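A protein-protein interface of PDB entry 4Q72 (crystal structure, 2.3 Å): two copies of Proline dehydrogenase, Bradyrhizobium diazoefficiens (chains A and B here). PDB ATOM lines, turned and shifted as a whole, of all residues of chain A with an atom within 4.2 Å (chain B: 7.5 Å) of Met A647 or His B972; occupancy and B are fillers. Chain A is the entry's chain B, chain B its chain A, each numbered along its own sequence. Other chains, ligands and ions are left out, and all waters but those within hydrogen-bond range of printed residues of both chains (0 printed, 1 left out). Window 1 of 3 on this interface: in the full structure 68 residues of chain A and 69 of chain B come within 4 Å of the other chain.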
ATOM      1  N   LEU A 628      21.313  -6.255  19.044  1.00  0.00           N
ATOM      2  CA  LEU A 628      20.187  -5.329  19.002  1.00  0.00           C
ATOM      3  C   LEU A 628      20.047  -4.558  17.665  1.00  0.00           C
ATOM      4  O   LEU A 628      18.953  -4.418  17.138  1.00  0.00           O
ATOM      5  CB  LEU A 628      20.292  -4.339  20.166  1.00  0.00           C
ATOM      6  CG  LEU A 628      19.036  -3.535  20.456  1.00  0.00           C
ATOM      7  CD1 LEU A 628      17.865  -4.497  20.538  1.00  0.00           C
ATOM      8  CD2 LEU A 628      19.189  -2.779  21.773  1.00  0.00           C
ATOM      9  N   PHE A 629      21.154  -4.051  17.137  1.00  0.00           N
ATOM     10  CA  PHE A 629      21.098  -3.167  15.978  1.00  0.00           C
ATOM     11  C   PHE A 629      21.666  -3.835  14.711  1.00  0.00           C
ATOM     12  O   PHE A 629      21.688  -3.236  13.640  1.00  0.00           O
ATOM     13  CB  PHE A 629      21.869  -1.877  16.282  1.00  0.00           C
ATOM     14  CG  PHE A 629      21.521  -1.259  17.617  1.00  0.00           C
ATOM     15  CD1 PHE A 629      22.495  -1.076  18.597  1.00  0.00           C
ATOM     16  CD2 PHE A 629      20.219  -0.841  17.889  1.00  0.00           C
ATOM     17  CE1 PHE A 629      22.178  -0.507  19.819  1.00  0.00           C
ATOM     18  CE2 PHE A 629      19.888  -0.262  19.114  1.00  0.00           C
ATOM     19  CZ  PHE A 629      20.866  -0.101  20.085  1.00  0.00           C
ATOM     20  N   LEU A 645      10.907  -4.629  12.264  1.00  0.00           N
ATOM     21  CA  LEU A 645      11.182  -3.692  13.345  1.00  0.00           C
ATOM     22  C   LEU A 645      12.677  -3.447  13.409  1.00  0.00           C
ATOM     23  O   LEU A 645      13.473  -4.383  13.379  1.00  0.00           O
ATOM     24  CB  LEU A 645      10.646  -4.239  14.684  1.00  0.00           C
ATOM     25  CG  LEU A 645      10.743  -3.345  15.928  1.00  0.00           C
ATOM     26  CD1 LEU A 645       9.937  -2.061  15.745  1.00  0.00           C
ATOM     27  CD2 LEU A 645      10.259  -4.092  17.163  1.00  0.00           C
ATOM     28  N   THR A 646      13.054  -2.178  13.454  1.00  0.00           N
ATOM     29  CA  THR A 646      14.457  -1.797  13.541  1.00  0.00           C
ATOM     30  C   THR A 646      14.647  -0.793  14.663  1.00  0.00           C
ATOM     31  O   THR A 646      13.679  -0.267  15.214  1.00  0.00           O
ATOM     32  CB  THR A 646      14.970  -1.171  12.241  1.00  0.00           C
ATOM     33  OG1 THR A 646      14.010  -0.228  11.760  1.00  0.00           O
ATOM     34  CG2 THR A 646      15.185  -2.232  11.195  1.00  0.00           C
ATOM     35  N   MET A 647      15.896  -0.539  15.014  1.00  0.00           N
ATOM     36  CA  MET A 647      16.192   0.434  16.052  1.00  0.00           C
ATOM     37  C   MET A 647      17.218   1.422  15.556  1.00  0.00           C
ATOM     38  O   MET A 647      18.313   1.037  15.174  1.00  0.00           O
ATOM     39  CB  MET A 647      16.760  -0.275  17.276  1.00  0.00           C
ATOM     40  CG  MET A 647      15.982  -1.494  17.678  1.00  0.00           C
ATOM     41  SD  MET A 647      14.771  -1.022  18.896  1.00  0.00           S
ATOM     42  CE  MET A 647      15.827  -0.966  20.325  1.00  0.00           C
ATOM     43  N   ARG A 648      16.895   2.703  15.627  1.00  0.00           N
ATOM     44  CA  ARG A 648      17.752   3.714  15.037  1.00  0.00           C
ATOM     45  C   ARG A 648      18.269   4.652  16.115  1.00  0.00           C
ATOM     46  O   ARG A 648      17.652   4.792  17.171  1.00  0.00           O
ATOM     47  CB  ARG A 648      16.963   4.517  14.007  1.00  0.00           C
ATOM     48  CG  ARG A 648      16.353   3.682  12.892  1.00  0.00           C
ATOM     49  CD  ARG A 648      15.550   4.565  11.945  1.00  0.00           C
ATOM     50  NE  ARG A 648      16.402   5.574  11.318  1.00  0.00           N
ATOM     51  CZ  ARG A 648      16.367   5.906  10.028  1.00  0.00           C
ATOM     52  NH1 ARG A 648      17.202   6.835   9.571  1.00  0.00           N
ATOM     53  NH2 ARG A 648      15.502   5.318   9.195  1.00  0.00           N
ATOM     54  N   ALA A 975      18.845  -0.220  24.256  1.00  0.00           N
ATOM     55  CA  ALA A 975      17.546   0.104  23.654  1.00  0.00           C
ATOM     56  C   ALA A 975      17.053   1.491  24.039  1.00  0.00           C
ATOM     57  O   ALA A 975      16.408   2.180  23.242  1.00  0.00           O
ATOM     58  CB  ALA A 975      16.498  -0.942  24.015  1.00  0.00           C
ATOM     59  N   THR A 979      15.574   4.514  19.013  1.00  0.00           N
ATOM     60  CA  THR A 979      14.140   4.574  18.774  1.00  0.00           C
ATOM     61  C   THR A 979      13.761   3.462  17.815  1.00  0.00           C
ATOM     62  O   THR A 979      14.567   3.064  16.989  1.00  0.00           O
ATOM     63  CB  THR A 979      13.678   5.996  18.303  1.00  0.00           C
ATOM     64  OG1 THR A 979      12.253   6.041  18.212  1.00  0.00           O
ATOM     65  CG2 THR A 979      14.266   6.371  16.956  1.00  0.00           C
ATOM     66  N   GLU A 980      12.541   2.951  17.945  1.00  0.00           N
ATOM     67  CA  GLU A 980      12.054   1.873  17.100  1.00  0.00           C
ATOM     68  C   GLU A 980      11.437   2.426  15.800  1.00  0.00           C
ATOM     69  O   GLU A 980      10.861   3.505  15.786  1.00  0.00           O
ATOM     70  CB  GLU A 980      10.986   1.055  17.817  1.00  0.00           C
ATOM     71  CG  GLU A 980      11.396   0.382  19.097  1.00  0.00           C
ATOM     72  CD  GLU A 980      10.180   0.020  19.944  1.00  0.00           C
ATOM     73  OE1 GLU A 980       9.585  -1.052  19.709  1.00  0.00           O
ATOM     74  OE2 GLU A 980       9.808   0.813  20.833  1.00  0.00           O
ATOM     75  N   TYR B 620      -1.390 -10.532  23.671  1.00  0.00           N
ATOM     76  CA  TYR B 620      -0.023 -10.232  23.307  1.00  0.00           C
ATOM     77  C   TYR B 620       0.830  -9.831  24.493  1.00  0.00           C
ATOM     78  O   TYR B 620       1.939 -10.329  24.659  1.00  0.00           O
ATOM     79  CB  TYR B 620       0.019  -9.094  22.297  1.00  0.00           C
ATOM     80  CG  TYR B 620       1.431  -8.713  21.931  1.00  0.00           C
ATOM     81  CD1 TYR B 620       2.223  -9.568  21.147  1.00  0.00           C
ATOM     82  CD2 TYR B 620       1.990  -7.514  22.367  1.00  0.00           C
ATOM     83  CE1 TYR B 620       3.537  -9.220  20.795  1.00  0.00           C
ATOM     84  CE2 TYR B 620       3.297  -7.157  22.005  1.00  0.00           C
ATOM     85  CZ  TYR B 620       4.055  -8.021  21.218  1.00  0.00           C
ATOM     86  OH  TYR B 620       5.344  -7.687  20.896  1.00  0.00           O
ATOM     87  N   GLN B 624       3.997 -11.786  25.979  1.00  0.00           N
ATOM     88  CA  GLN B 624       5.261 -11.088  26.220  1.00  0.00           C
ATOM     89  C   GLN B 624       5.536 -11.047  27.727  1.00  0.00           C
ATOM     90  O   GLN B 624       6.684 -11.125  28.161  1.00  0.00           O
ATOM     91  CB  GLN B 624       5.235  -9.659  25.649  1.00  0.00           C
ATOM     92  CG  GLN B 624       5.115  -9.576  24.106  1.00  0.00           C
ATOM     93  CD  GLN B 624       6.335 -10.152  23.398  1.00  0.00           C
ATOM     94  OE1 GLN B 624       6.233 -11.088  22.606  1.00  0.00           O
ATOM     95  NE2 GLN B 624       7.500  -9.584  23.682  1.00  0.00           N
ATOM     96  N   LEU B 628       8.901 -12.203  29.544  1.00  0.00           N
ATOM     97  CA  LEU B 628       9.692 -11.187  30.216  1.00  0.00           C
ATOM     98  C   LEU B 628       9.773 -11.381  31.740  1.00  0.00           C
ATOM     99  O   LEU B 628      10.842 -11.238  32.319  1.00  0.00           O
ATOM    100  CB  LEU B 628       9.151  -9.796  29.896  1.00  0.00           C
ATOM    101  CG  LEU B 628      10.090  -8.675  30.326  1.00  0.00           C
ATOM    102  CD1 LEU B 628      11.494  -8.973  29.814  1.00  0.00           C
ATOM    103  CD2 LEU B 628       9.607  -7.312  29.818  1.00  0.00           C
ATOM    104  N   ILE B 758       5.532   7.514  29.627  1.00  0.00           N
ATOM    105  CA  ILE B 758       5.296   6.993  28.287  1.00  0.00           C
ATOM    106  C   ILE B 758       4.157   7.791  27.696  1.00  0.00           C
ATOM    107  O   ILE B 758       3.027   7.736  28.193  1.00  0.00           O
ATOM    108  CB  ILE B 758       4.903   5.506  28.299  1.00  0.00           C
ATOM    109  CG1 ILE B 758       6.042   4.662  28.862  1.00  0.00           C
ATOM    110  CG2 ILE B 758       4.522   5.023  26.886  1.00  0.00           C
ATOM    111  CD1 ILE B 758       5.587   3.306  29.409  1.00  0.00           C
ATOM    112  N   PRO B 955       4.210  -2.849  15.533  1.00  0.00           N
ATOM    113  CA  PRO B 955       4.426  -2.076  16.766  1.00  0.00           C
ATOM    114  C   PRO B 955       4.255  -0.587  16.467  1.00  0.00           C
ATOM    115  O   PRO B 955       4.960  -0.028  15.632  1.00  0.00           O
ATOM    116  CB  PRO B 955       5.882  -2.399  17.127  1.00  0.00           C
ATOM    117  CG  PRO B 955       6.052  -3.824  16.633  1.00  0.00           C
ATOM    118  CD  PRO B 955       5.230  -3.905  15.356  1.00  0.00           C
ATOM    119  N   GLY B 965       8.167   6.733  23.045  1.00  0.00           N
ATOM    120  CA  GLY B 965       8.483   5.316  23.059  1.00  0.00           C
ATOM    121  C   GLY B 965       8.237   4.798  24.482  1.00  0.00           C
ATOM    122  O   GLY B 965       7.920   5.585  25.385  1.00  0.00           O
ATOM    123  N   PRO B 966       8.310   3.473  24.682  1.00  0.00           N
ATOM    124  CA  PRO B 966       8.482   2.479  23.614  1.00  0.00           C
ATOM    125  C   PRO B 966       7.163   2.289  22.832  1.00  0.00           C
ATOM    126  O   PRO B 966       6.125   2.839  23.201  1.00  0.00           O
ATOM    127  CB  PRO B 966       8.853   1.206  24.390  1.00  0.00           C
ATOM    128  CG  PRO B 966       8.172   1.383  25.721  1.00  0.00           C
ATOM    129  CD  PRO B 966       8.261   2.853  26.025  1.00  0.00           C
ATOM    130  N   LYS B 967       7.223   1.540  21.742  1.00  0.00           N
ATOM    131  CA  LYS B 967       6.055   1.300  20.908  1.00  0.00           C
ATOM    132  C   LYS B 967       5.063   0.335  21.572  1.00  0.00           C
ATOM    133  O   LYS B 967       5.429  -0.775  21.954  1.00  0.00           O
ATOM    134  CB  LYS B 967       6.478   0.710  19.556  1.00  0.00           C
ATOM    135  CG  LYS B 967       7.148   1.648  18.547  1.00  0.00           C
ATOM    136  CD  LYS B 967       7.616   0.785  17.366  1.00  0.00           C
ATOM    137  CE  LYS B 967       7.938   1.569  16.062  1.00  0.00           C
ATOM    138  NZ  LYS B 967       6.731   2.009  15.346  1.00  0.00           N
ATOM    139  N   ALA B 968       3.809   0.761  21.685  1.00  0.00           N
ATOM    140  CA  ALA B 968       2.726  -0.116  22.110  1.00  0.00           C
ATOM    141  C   ALA B 968       2.547  -1.258  21.106  1.00  0.00           C
ATOM    142  O   ALA B 968       2.783  -1.092  19.910  1.00  0.00           O
ATOM    143  CB  ALA B 968       1.413   0.686  22.253  1.00  0.00           C
ATOM    144  N   GLY B 969       2.156  -2.428  21.601  1.00  0.00           N
ATOM    145  CA  GLY B 969       1.916  -3.579  20.749  1.00  0.00           C
ATOM    146  C   GLY B 969       3.191  -4.185  20.178  1.00  0.00           C
ATOM    147  O   GLY B 969       3.116  -5.038  19.291  1.00  0.00           O
ATOM    148  N   GLY B 970       4.348  -3.738  20.679  1.00  0.00           N
ATOM    149  CA  GLY B 970       5.651  -4.249  20.276  1.00  0.00           C
ATOM    150  C   GLY B 970       6.444  -4.869  21.437  1.00  0.00           C
ATOM    151  O   GLY B 970       6.012  -4.835  22.585  1.00  0.00           O
ATOM    152  N   PRO B 971       7.620  -5.434  21.147  1.00  0.00           N
ATOM    153  CA  PRO B 971       8.337  -6.223  22.165  1.00  0.00           C
ATOM    154  C   PRO B 971       9.196  -5.419  23.143  1.00  0.00           C
ATOM    155  O   PRO B 971       9.888  -6.028  23.957  1.00  0.00           O
ATOM    156  CB  PRO B 971       9.239  -7.134  21.320  1.00  0.00           C
ATOM    157  CG  PRO B 971       9.539  -6.294  20.093  1.00  0.00           C
ATOM    158  CD  PRO B 971       8.226  -5.568  19.810  1.00  0.00           C
ATOM    159  N   HIS B 972       9.161  -4.096  23.084  1.00  0.00           N
ATOM    160  CA  HIS B 972       9.966  -3.290  24.006  1.00  0.00           C
ATOM    161  C   HIS B 972       9.076  -2.523  24.976  1.00  0.00           C
ATOM    162  O   HIS B 972       9.548  -1.711  25.766  1.00  0.00           O
ATOM    163  CB  HIS B 972      10.863  -2.303  23.251  1.00  0.00           C
ATOM    164  CG  HIS B 972      11.869  -2.963  22.367  1.00  0.00           C
ATOM    165  ND1 HIS B 972      11.606  -3.295  21.053  1.00  0.00           N
ATOM    166  CD2 HIS B 972      13.139  -3.359  22.609  1.00  0.00           C
ATOM    167  CE1 HIS B 972      12.672  -3.871  20.524  1.00  0.00           C
ATOM    168  NE2 HIS B 972      13.617  -3.919  21.447  1.00  0.00           N
ATOM    169  N   TYR B 973       7.782  -2.803  24.921  1.00  0.00           N
ATOM    170  CA  TYR B 973       6.815  -2.013  25.669  1.00  0.00           C
ATOM    171  C   TYR B 973       6.761  -2.361  27.157  1.00  0.00           C
ATOM    172  O   TYR B 973       6.837  -1.487  27.982  1.00  0.00           O
ATOM    173  CB  TYR B 973       5.444  -2.194  25.050  1.00  0.00           C
ATOM    174  CG  TYR B 973       4.402  -1.177  25.453  1.00  0.00           C
ATOM    175  CD1 TYR B 973       4.561   0.177  25.155  1.00  0.00           C
ATOM    176  CD2 TYR B 973       3.218  -1.586  26.074  1.00  0.00           C
ATOM    177  CE1 TYR B 973       3.576   1.095  25.492  1.00  0.00           C
ATOM    178  CE2 TYR B 973       2.236  -0.685  26.405  1.00  0.00           C
ATOM    179  CZ  TYR B 973       2.417   0.654  26.108  1.00  0.00           C
ATOM    180  OH  TYR B 973       1.435   1.542  26.454  1.00  0.00           O
ATOM    181  N   LEU B 974       6.609  -3.641  27.474  1.00  0.00           N
ATOM    182  CA  LEU B 974       6.409  -4.096  28.844  1.00  0.00           C
ATOM    183  C   LEU B 974       7.556  -3.746  29.799  1.00  0.00           C
ATOM    184  O   LEU B 974       7.316  -3.344  30.936  1.00  0.00           O
ATOM    185  CB  LEU B 974       6.125  -5.596  28.867  1.00  0.00           C
ATOM    186  CG  LEU B 974       4.751  -6.053  28.365  1.00  0.00           C
ATOM    187  CD1 LEU B 974       4.546  -7.530  28.579  1.00  0.00           C
ATOM    188  CD2 LEU B 974       3.643  -5.309  29.062  1.00  0.00           C
ATOM    189  N   ALA B 975       8.787  -3.899  29.329  1.00  0.00           N
ATOM    190  CA  ALA B 975       9.976  -3.650  30.135  1.00  0.00           C
ATOM    191  C   ALA B 975       9.984  -2.259  30.762  1.00  0.00           C
ATOM    192  O   ALA B 975      10.421  -2.071  31.903  1.00  0.00           O
ATOM    193  CB  ALA B 975      11.229  -3.851  29.298  1.00  0.00           C
ATOM    194  N   ARG B 976       9.457  -1.288  30.020  1.00  0.00           N
ATOM    195  CA  ARG B 976       9.458   0.096  30.470  1.00  0.00           C
ATOM    196  C   ARG B 976       8.579   0.309  31.713  1.00  0.00           C
ATOM    197  O   ARG B 976       8.774   1.276  32.439  1.00  0.00           O
ATOM    198  CB  ARG B 976       9.002   1.004  29.337  1.00  0.00           C
ATOM    199  CG  ARG B 976       9.172   2.473  29.609  1.00  0.00           C
ATOM    200  CD  ARG B 976      10.615   2.927  29.461  1.00  0.00           C
ATOM    201  NE  ARG B 976      10.612   4.382  29.466  1.00  0.00           N
ATOM    202  CZ  ARG B 976      11.034   5.138  30.476  1.00  0.00           C
ATOM    203  NH1 ARG B 976      10.956   6.461  30.385  1.00  0.00           N
ATOM    204  NH2 ARG B 976      11.530   4.579  31.568  1.00  0.00           N
ATOM    205  N   PHE B 977       7.625  -0.601  31.947  1.00  0.00           N
ATOM    206  CA  PHE B 977       6.705  -0.503  33.076  1.00  0.00           C
ATOM    207  C   PHE B 977       7.277  -1.155  34.330  1.00  0.00           C
ATOM    208  O   PHE B 977       6.623  -1.178  35.381  1.00  0.00           O
ATOM    209  CB  PHE B 977       5.365  -1.183  32.765  1.00  0.00           C
ATOM    210  CG  PHE B 977       4.509  -0.449  31.763  1.00  0.00           C
ATOM    211  CD1 PHE B 977       4.669  -0.670  30.390  1.00  0.00           C
ATOM    212  CD2 PHE B 977       3.529   0.447  32.187  1.00  0.00           C
ATOM    213  CE1 PHE B 977       3.864  -0.019  29.460  1.00  0.00           C
ATOM    214  CE2 PHE B 977       2.725   1.120  31.254  1.00  0.00           C
ATOM    215  CZ  PHE B 977       2.898   0.883  29.898  1.00  0.00           C
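The side-chain carboxylate of Glu A980 is in hydrogen-bond range of the backbone NH of Lys B967 (2.8 Å). ND1 of His B972 is in hydrogen-bond range of OE1 of Glu A980, 3.3 Å away.
NZ of Lys B967 lies within hydrogen-bond range of O of Pro B955, at 2.7 Å.
Among the printed residues, pairs that only touch across the chains: Leu A645 with Pro B971, Met A647 with His B972 and Glu A980 with Pro B966.
Of chain A, only Met A647 (3.9 Å) and Glu A980 (3.3 Å) come within 4 Å of His B972. Of the printed residues of chain A, Pro B966 touches Glu A980. Of the printed residues of chain B, Glu A980 touches Pro B966 (3.5 Å), Lys B967 (2.8 Å) and His B972 (3.3 Å). Of the printed residues of chain B, Leu A645 touches Pro B971. Tyr B620 touches none of the printed residues of chain A. Ala B975 touches none of the printed residues of chain A. The nearest residue of chain A that does not touch His B972 is Leu A645 (4.1 Å). The nearest printed residue of chain A that does not touch Pro B966 is Thr A979 (7.5 Å).
Of the 9 printed residues of chain A, 3 touch a printed residue of chain B. Printed residues of chain A that touch a printed residue of chain B: Leu A645, Met A647 and Glu A980. Hydrophobic or aromatic side chains of chain A that line the printed part of chain B: Leu A645 and Met A647. Among the printed residues, 5 pairs touch across the chains.
Positions printed for both chains: 628 and 975.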
